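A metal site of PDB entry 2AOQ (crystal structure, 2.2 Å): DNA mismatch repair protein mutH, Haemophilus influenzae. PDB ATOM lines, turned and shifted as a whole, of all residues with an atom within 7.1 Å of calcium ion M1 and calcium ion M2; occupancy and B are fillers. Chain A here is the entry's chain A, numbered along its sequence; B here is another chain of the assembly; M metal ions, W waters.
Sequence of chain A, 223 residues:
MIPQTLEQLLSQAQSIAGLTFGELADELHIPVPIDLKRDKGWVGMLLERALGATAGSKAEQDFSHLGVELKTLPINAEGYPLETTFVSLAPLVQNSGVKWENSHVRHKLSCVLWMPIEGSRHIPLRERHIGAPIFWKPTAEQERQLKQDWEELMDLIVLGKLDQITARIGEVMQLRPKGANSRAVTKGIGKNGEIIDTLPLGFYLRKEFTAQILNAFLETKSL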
ATOM      1  N   GLY A  44     -23.388  21.698   4.506  1.00  0.00           N
ATOM      2  CA  GLY A  44     -22.002  22.100   4.645  1.00  0.00           C
ATOM      3  C   GLY A  44     -21.933  23.502   5.194  1.00  0.00           C
ATOM      4  O   GLY A  44     -21.210  23.785   6.136  1.00  0.00           O
ATOM      5  N   MET A  45     -22.722  24.403   4.620  1.00  0.00           N
ATOM      6  CA  MET A  45     -22.705  25.780   5.062  1.00  0.00           C
ATOM      7  C   MET A  45     -23.240  25.950   6.475  1.00  0.00           C
ATOM      8  O   MET A  45     -22.773  26.802   7.248  1.00  0.00           O
ATOM      9  CB  MET A  45     -23.504  26.652   4.104  1.00  0.00           C
ATOM     10  CG  MET A  45     -22.890  26.735   2.679  1.00  0.00           C
ATOM     11  SD  MET A  45     -21.076  27.143   2.692  1.00  0.00           S
ATOM     12  CE  MET A  45     -20.759  27.957   1.016  1.00  0.00           C
ATOM     13  N   GLU A  48     -20.444  25.299   8.707  1.00  0.00           N
ATOM     14  CA  GLU A  48     -19.422  26.339   8.699  1.00  0.00           C
ATOM     15  C   GLU A  48     -19.805  27.476   9.644  1.00  0.00           C
ATOM     16  O   GLU A  48     -19.001  27.950  10.450  1.00  0.00           O
ATOM     17  CB  GLU A  48     -19.208  26.878   7.290  1.00  0.00           C
ATOM     18  CG  GLU A  48     -18.567  25.890   6.347  1.00  0.00           C
ATOM     19  CD  GLU A  48     -18.007  26.565   5.109  1.00  0.00           C
ATOM     20  OE1 GLU A  48     -18.736  27.377   4.507  1.00  0.00           O
ATOM     21  OE2 GLU A  48     -16.854  26.271   4.739  1.00  0.00           O
ATOM     22  N   ALA A  53     -16.246  28.766  10.792  1.00  0.00           N
ATOM     23  CA  ALA A  53     -15.302  28.512   9.711  1.00  0.00           C
ATOM     24  C   ALA A  53     -15.400  29.590   8.631  1.00  0.00           C
ATOM     25  O   ALA A  53     -16.364  30.360   8.588  1.00  0.00           O
ATOM     26  CB  ALA A  53     -15.569  27.149   9.091  1.00  0.00           C
ATOM     27  N   THR A  54     -14.390  29.640   7.761  1.00  0.00           N
ATOM     28  CA  THR A  54     -14.365  30.609   6.664  1.00  0.00           C
ATOM     29  C   THR A  54     -15.460  30.254   5.662  1.00  0.00           C
ATOM     30  O   THR A  54     -15.511  29.122   5.161  1.00  0.00           O
ATOM     31  CB  THR A  54     -13.012  30.602   5.922  1.00  0.00           C
ATOM     32  OG1 THR A  54     -11.930  30.693   6.854  1.00  0.00           O
ATOM     33  CG2 THR A  54     -12.922  31.786   4.969  1.00  0.00           C
ATOM     34  N   ALA A  55     -16.338  31.213   5.381  1.00  0.00           N
ATOM     35  CA  ALA A  55     -17.419  31.017   4.421  1.00  0.00           C
ATOM     36  C   ALA A  55     -16.940  31.435   3.044  1.00  0.00           C
ATOM     37  O   ALA A  55     -15.746  31.632   2.823  1.00  0.00           O
ATOM     38  CB  ALA A  55     -18.639  31.841   4.833  1.00  0.00           C
ATOM     39  N   GLY A  56     -17.884  31.561   2.118  1.00  0.00           N
ATOM     40  CA  GLY A  56     -17.542  31.985   0.773  1.00  0.00           C
ATOM     41  C   GLY A  56     -16.556  31.094   0.040  1.00  0.00           C
ATOM     42  O   GLY A  56     -16.331  29.934   0.416  1.00  0.00           O
ATOM     43  N   SER A  57     -15.951  31.645  -1.007  1.00  0.00           N
ATOM     44  CA  SER A  57     -14.989  30.902  -1.813  1.00  0.00           C
ATOM     45  C   SER A  57     -13.548  31.091  -1.356  1.00  0.00           C
ATOM     46  O   SER A  57     -12.608  30.898  -2.138  1.00  0.00           O
ATOM     47  CB  SER A  57     -15.147  31.314  -3.279  1.00  0.00           C
ATOM     48  OG  SER A  57     -16.497  31.188  -3.707  1.00  0.00           O
ATOM     49  N   LYS A  58     -13.368  31.475  -0.091  1.00  0.00           N
ATOM     50  CA  LYS A  58     -12.019  31.659   0.448  1.00  0.00           C
ATOM     51  C   LYS A  58     -11.255  30.374   0.178  1.00  0.00           C
ATOM     52  O   LYS A  58     -11.663  29.293   0.613  1.00  0.00           O
ATOM     53  CB  LYS A  58     -12.086  31.943   1.947  1.00  0.00           C
ATOM     54  N   GLU A  60      -9.114  27.095  -0.170  1.00  0.00           N
ATOM     55  CA  GLU A  60      -8.727  25.887   0.557  1.00  0.00           C
ATOM     56  C   GLU A  60      -8.728  25.699   2.074  1.00  0.00           C
ATOM     57  O   GLU A  60      -8.405  24.599   2.522  1.00  0.00           O
ATOM     58  CB  GLU A  60      -7.374  25.409   0.021  1.00  0.00           C
ATOM     59  N   GLN A  61      -9.042  26.707   2.889  1.00  0.00           N
ATOM     60  CA  GLN A  61      -9.021  26.388   4.317  1.00  0.00           C
ATOM     61  C   GLN A  61      -9.934  27.110   5.313  1.00  0.00           C
ATOM     62  O   GLN A  61      -9.821  28.311   5.561  1.00  0.00           O
ATOM     63  CB  GLN A  61      -7.576  26.351   4.831  1.00  0.00           C
ATOM     64  CG  GLN A  61      -7.129  24.897   5.063  1.00  0.00           C
ATOM     65  CD  GLN A  61      -5.693  24.734   5.503  1.00  0.00           C
ATOM     66  OE1 GLN A  61      -5.120  25.601   6.170  1.00  0.00           O
ATOM     67  NE2 GLN A  61      -5.101  23.590   5.152  1.00  0.00           N
ATOM     68  N   ASP A  62     -10.817  26.306   5.881  1.00  0.00           N
ATOM     69  CA  ASP A  62     -11.808  26.731   6.862  1.00  0.00           C
ATOM     70  C   ASP A  62     -11.202  27.336   8.122  1.00  0.00           C
ATOM     71  O   ASP A  62     -11.702  28.332   8.643  1.00  0.00           O
ATOM     72  CB  ASP A  62     -12.701  25.531   7.228  1.00  0.00           C
ATOM     73  CG  ASP A  62     -13.325  24.872   6.004  1.00  0.00           C
ATOM     74  OD1 ASP A  62     -13.995  25.588   5.221  1.00  0.00           O
ATOM     75  OD2 ASP A  62     -13.149  23.651   5.830  1.00  0.00           O
ATOM     76  N   PHE A  63     -10.125  26.737   8.632  1.00  0.00           N
ATOM     77  CA  PHE A  63      -9.479  27.261   9.826  1.00  0.00           C
ATOM     78  C   PHE A  63      -7.980  27.367   9.555  1.00  0.00           C
ATOM     79  O   PHE A  63      -7.170  26.598  10.090  1.00  0.00           O
ATOM     80  CB  PHE A  63      -9.751  26.336  11.022  1.00  0.00           C
ATOM     81  CG  PHE A  63     -11.201  26.047  11.249  1.00  0.00           C
ATOM     82  CD1 PHE A  63     -11.770  24.852  10.800  1.00  0.00           C
ATOM     83  CD2 PHE A  63     -12.013  26.963  11.917  1.00  0.00           C
ATOM     84  CE1 PHE A  63     -13.121  24.576  11.009  1.00  0.00           C
ATOM     85  CE2 PHE A  63     -13.368  26.702  12.137  1.00  0.00           C
ATOM     86  CZ  PHE A  63     -13.925  25.503  11.681  1.00  0.00           C
ATOM     87  N   VAL A  68      -6.967  23.410   9.811  1.00  0.00           N
ATOM     88  CA  VAL A  68      -7.977  22.372   9.766  1.00  0.00           C
ATOM     89  C   VAL A  68      -8.983  22.619   8.666  1.00  0.00           C
ATOM     90  O   VAL A  68      -9.391  23.757   8.435  1.00  0.00           O
ATOM     91  CB  VAL A  68      -8.712  22.256  11.106  1.00  0.00           C
ATOM     92  CG1 VAL A  68      -9.829  21.219  11.005  1.00  0.00           C
ATOM     93  CG2 VAL A  68      -7.740  21.864  12.205  1.00  0.00           C
ATOM     94  N   GLU A  69      -9.364  21.539   7.979  1.00  0.00           N
ATOM     95  CA  GLU A  69     -10.358  21.557   6.906  1.00  0.00           C
ATOM     96  C   GLU A  69     -11.616  20.875   7.436  1.00  0.00           C
ATOM     97  O   GLU A  69     -11.548  19.776   7.971  1.00  0.00           O
ATOM     98  CB  GLU A  69      -9.863  20.782   5.682  1.00  0.00           C
ATOM     99  CG  GLU A  69     -10.913  20.560   4.595  1.00  0.00           C
ATOM    100  CD  GLU A  69     -11.347  21.845   3.883  1.00  0.00           C
ATOM    101  OE1 GLU A  69     -12.409  21.828   3.224  1.00  0.00           O
ATOM    102  OE2 GLU A  69     -10.617  22.873   3.970  1.00  0.00           O
ATOM    103  N   LEU A  70     -12.761  21.533   7.296  1.00  0.00           N
ATOM    104  CA  LEU A  70     -14.019  20.971   7.764  1.00  0.00           C
ATOM    105  C   LEU A  70     -14.774  20.298   6.619  1.00  0.00           C
ATOM    106  O   LEU A  70     -14.857  20.814   5.509  1.00  0.00           O
ATOM    107  CB  LEU A  70     -14.888  22.096   8.347  1.00  0.00           C
ATOM    108  CG  LEU A  70     -16.319  21.747   8.753  1.00  0.00           C
ATOM    109  CD1 LEU A  70     -16.298  20.859   9.980  1.00  0.00           C
ATOM    110  CD2 LEU A  70     -17.091  23.032   9.038  1.00  0.00           C
ATOM    111  N   LYS A  71     -15.309  19.104   6.887  1.00  0.00           N
ATOM    112  CA  LYS A  71     -16.078  18.382   5.878  1.00  0.00           C
ATOM    113  C   LYS A  71     -17.221  17.588   6.467  1.00  0.00           C
ATOM    114  O   LYS A  71     -17.033  16.851   7.413  1.00  0.00           O
ATOM    115  CB  LYS A  71     -15.175  17.425   5.088  1.00  0.00           C
ATOM    116  CG  LYS A  71     -14.284  18.131   4.098  1.00  0.00           C
ATOM    117  CD  LYS A  71     -13.619  17.136   3.155  1.00  0.00           C
ATOM    118  CE  LYS A  71     -12.923  17.881   2.042  1.00  0.00           C
ATOM    119  NZ  LYS A  71     -13.876  18.822   1.409  1.00  0.00           N
ATOM    120  N   THR A  72     -18.424  17.766   5.908  1.00  0.00           N
ATOM    121  CA  THR A  72     -19.581  17.011   6.365  1.00  0.00           C
ATOM    122  C   THR A  72     -19.505  15.665   5.646  1.00  0.00           C
ATOM    123  O   THR A  72     -18.896  15.575   4.588  1.00  0.00           O
ATOM    124  CB  THR A  72     -20.902  17.682   5.969  1.00  0.00           C
ATOM    125  OG1 THR A  72     -20.861  17.993   4.574  1.00  0.00           O
ATOM    126  CG2 THR A  72     -21.136  18.945   6.786  1.00  0.00           C
ATOM    127  P    DT B   4     -11.698  25.692  -3.064  1.00  0.00           P
ATOM    128  OP1  DT B   4     -10.545  25.670  -2.143  1.00  0.00           O
ATOM    129  OP2  DT B   4     -11.952  24.524  -3.954  1.00  0.00           O
ATOM    130  O5'  DT B   4     -13.033  25.952  -2.249  1.00  0.00           O
ATOM    131  C5'  DT B   4     -13.211  27.167  -1.521  1.00  0.00           C
ATOM    132  C4'  DT B   4     -14.673  27.369  -1.198  1.00  0.00           C
ATOM    133  O4'  DT B   4     -15.401  27.722  -2.404  1.00  0.00           O
ATOM    134  C3'  DT B   4     -15.419  26.161  -0.683  1.00  0.00           C
ATOM    135  O3'  DT B   4     -15.164  25.919   0.700  1.00  0.00           O
ATOM    136  C2'  DT B   4     -16.869  26.571  -0.930  1.00  0.00           C
ATOM    137  C1'  DT B   4     -16.760  27.323  -2.255  1.00  0.00           C
ATOM    138  N1   DT B   4     -17.137  26.488  -3.411  1.00  0.00           N
ATOM    139  C2   DT B   4     -18.453  26.503  -3.778  1.00  0.00           C
ATOM    140  O2   DT B   4     -19.295  27.169  -3.190  1.00  0.00           O
ATOM    141  N3   DT B   4     -18.765  25.711  -4.848  1.00  0.00           N
ATOM    142  C4   DT B   4     -17.911  24.914  -5.582  1.00  0.00           C
ATOM    143  O4   DT B   4     -18.343  24.265  -6.542  1.00  0.00           O
ATOM    144  C5   DT B   4     -16.521  24.944  -5.129  1.00  0.00           C
ATOM    145  C7   DT B   4     -15.522  24.087  -5.834  1.00  0.00           C
ATOM    146  C6   DT B   4     -16.210  25.723  -4.093  1.00  0.00           C
ATOM    147  P    DG B   5     -15.147  24.400   1.245  1.00  0.00           P
ATOM    148  OP1  DG B   5     -14.910  24.449   2.704  1.00  0.00           O
ATOM    149  OP2  DG B   5     -14.246  23.589   0.372  1.00  0.00           O
ATOM    150  O5'  DG B   5     -16.640  23.903   1.028  1.00  0.00           O
ATOM    151  C5'  DG B   5     -17.706  24.524   1.726  1.00  0.00           C
ATOM    152  C4'  DG B   5     -19.036  23.950   1.286  1.00  0.00           C
ATOM    153  O4'  DG B   5     -19.398  24.392  -0.045  1.00  0.00           O
ATOM    154  C3'  DG B   5     -19.166  22.444   1.180  1.00  0.00           C
ATOM    155  O3'  DG B   5     -19.264  21.894   2.488  1.00  0.00           O
ATOM    156  C2'  DG B   5     -20.474  22.310   0.408  1.00  0.00           C
ATOM    157  C1'  DG B   5     -20.414  23.524  -0.527  1.00  0.00           C
ATOM    158  N9   DG B   5     -20.099  23.125  -1.884  1.00  0.00           N
ATOM    159  C8   DG B   5     -18.895  22.666  -2.375  1.00  0.00           C
ATOM    160  N7   DG B   5     -18.979  22.263  -3.615  1.00  0.00           N
ATOM    161  C5   DG B   5     -20.293  22.490  -3.965  1.00  0.00           C
ATOM    162  C6   DG B   5     -20.977  22.242  -5.173  1.00  0.00           C
ATOM    163  O6   DG B   5     -20.549  21.708  -6.212  1.00  0.00           O
ATOM    164  N1   DG B   5     -22.302  22.657  -5.119  1.00  0.00           N
ATOM    165  C2   DG B   5     -22.896  23.231  -4.017  1.00  0.00           C
ATOM    166  N2   DG B   5     -24.199  23.589  -4.142  1.00  0.00           N
ATOM    167  N3   DG B   5     -22.274  23.443  -2.868  1.00  0.00           N
ATOM    168  C4   DG B   5     -20.992  23.058  -2.924  1.00  0.00           C
ATOM    169  P    DA B   6     -19.150  20.315   2.711  1.00  0.00           P
ATOM    170  OP1  DA B   6     -19.345  20.071   4.170  1.00  0.00           O
ATOM    171  OP2  DA B   6     -17.939  19.810   2.040  1.00  0.00           O
ATOM    172  O5'  DA B   6     -20.454  19.763   1.966  1.00  0.00           O
ATOM    173  C5'  DA B   6     -20.401  18.688   1.051  1.00  0.00           C
ATOM    174  C4'  DA B   6     -21.563  18.808   0.094  1.00  0.00           C
ATOM    175  O4'  DA B   6     -21.135  19.433  -1.136  1.00  0.00           O
ATOM    176  C3'  DA B   6     -22.227  17.523  -0.348  1.00  0.00           C
ATOM    177  O3'  DA B   6     -23.166  17.154   0.644  1.00  0.00           O
ATOM    178  C2'  DA B   6     -22.949  17.973  -1.621  1.00  0.00           C
ATOM    179  C1'  DA B   6     -22.009  19.051  -2.167  1.00  0.00           C
ATOM    180  N9   DA B   6     -21.219  18.652  -3.325  1.00  0.00           N
ATOM    181  C8   DA B   6     -19.919  18.194  -3.432  1.00  0.00           C
ATOM    182  N7   DA B   6     -19.556  17.930  -4.663  1.00  0.00           N
ATOM    183  C5   DA B   6     -20.686  18.230  -5.423  1.00  0.00           C
ATOM    184  C6   DA B   6     -20.947  18.165  -6.795  1.00  0.00           C
ATOM    185  N6   DA B   6     -20.070  17.761  -7.706  1.00  0.00           N
ATOM    186  N1   DA B   6     -22.174  18.537  -7.214  1.00  0.00           N
ATOM    187  C2   DA B   6     -23.065  18.950  -6.304  1.00  0.00           C
ATOM    188  N3   DA B   6     -22.936  19.053  -4.993  1.00  0.00           N
ATOM    189  C4   DA B   6     -21.700  18.670  -4.610  1.00  0.00           C
HETATM  190 CA    CA M   1     -14.508  22.705   4.159  1.00  0.00          CA
HETATM  191 CA    CA M   2     -14.938  26.815   3.535  1.00  0.00          CA
HETATM  192  O   HOH W   1     -15.377  21.208   2.357  1.00  0.00           O
HETATM  193  O   HOH W   2     -16.794  27.885   2.479  1.00  0.00           O
HETATM  194  O   HOH W   3     -16.660  23.304   5.008  1.00  0.00           O
HETATM  195  O   HOH W   4     -12.762  27.054   2.833  1.00  0.00           O
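O of Glu 48 sits at hydrogen-bond distance from N of Ala 53. OE1 of Glu 69 lies close to NZ of Lys 71. OG1 of Thr 54 is in hydrogen-bond range of O of Gln 61 (3.4 Å). The backbone NH (N) of Glu 60 sits at hydrogen-bond distance from OP1 of DT 4 of chain B.
The nearest printed residue that does not touch calcium ion M1 is Glu 48 (4.3 Å).
Calcium ion M1 is bound by OP1 of DG 5 of chain B, O of Leu 70, OD2 of Asp 62, water W3, OE1 of Glu 69 and water W1. Calcium ion M1 has six donor atoms within binding distance. Slightly farther from calcium ion M1 lies the side-chain carboxylate (OD1) of Asp 62 (3.1 Å).
Calcium ion M2 is bound by OD1 of Asp 62, at 2.3 Å. Calcium ion M2 is bound by water W4, 2.3 Å away. OE2 of Glu 48 binds calcium ion M2 (2.3 Å). Calcium ion M2 is bound by water W2 (2.4 Å). OP1 of DG 5 of chain B is bound to calcium ion M2, 2.5 Å away. Calcium ion M2 is bound by the backbone carbonyl oxygen (O) of Thr 54 (2.9 Å). Calcium ion M2 has six donor atoms within binding distance. Slightly farther from calcium ion M2 lies O3' of DT 4 of chain B (3.0 Å).
Water W1 lies within hydrogen-bond range of OP2 of DA 6 of chain B, the side-chain amino group of Lys 71 and O5' of DG 5 of chain B. Water W4 bridges O of Lys 58 (3.3 Å) and O3' of DT 4 of chain B (3.4 Å).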
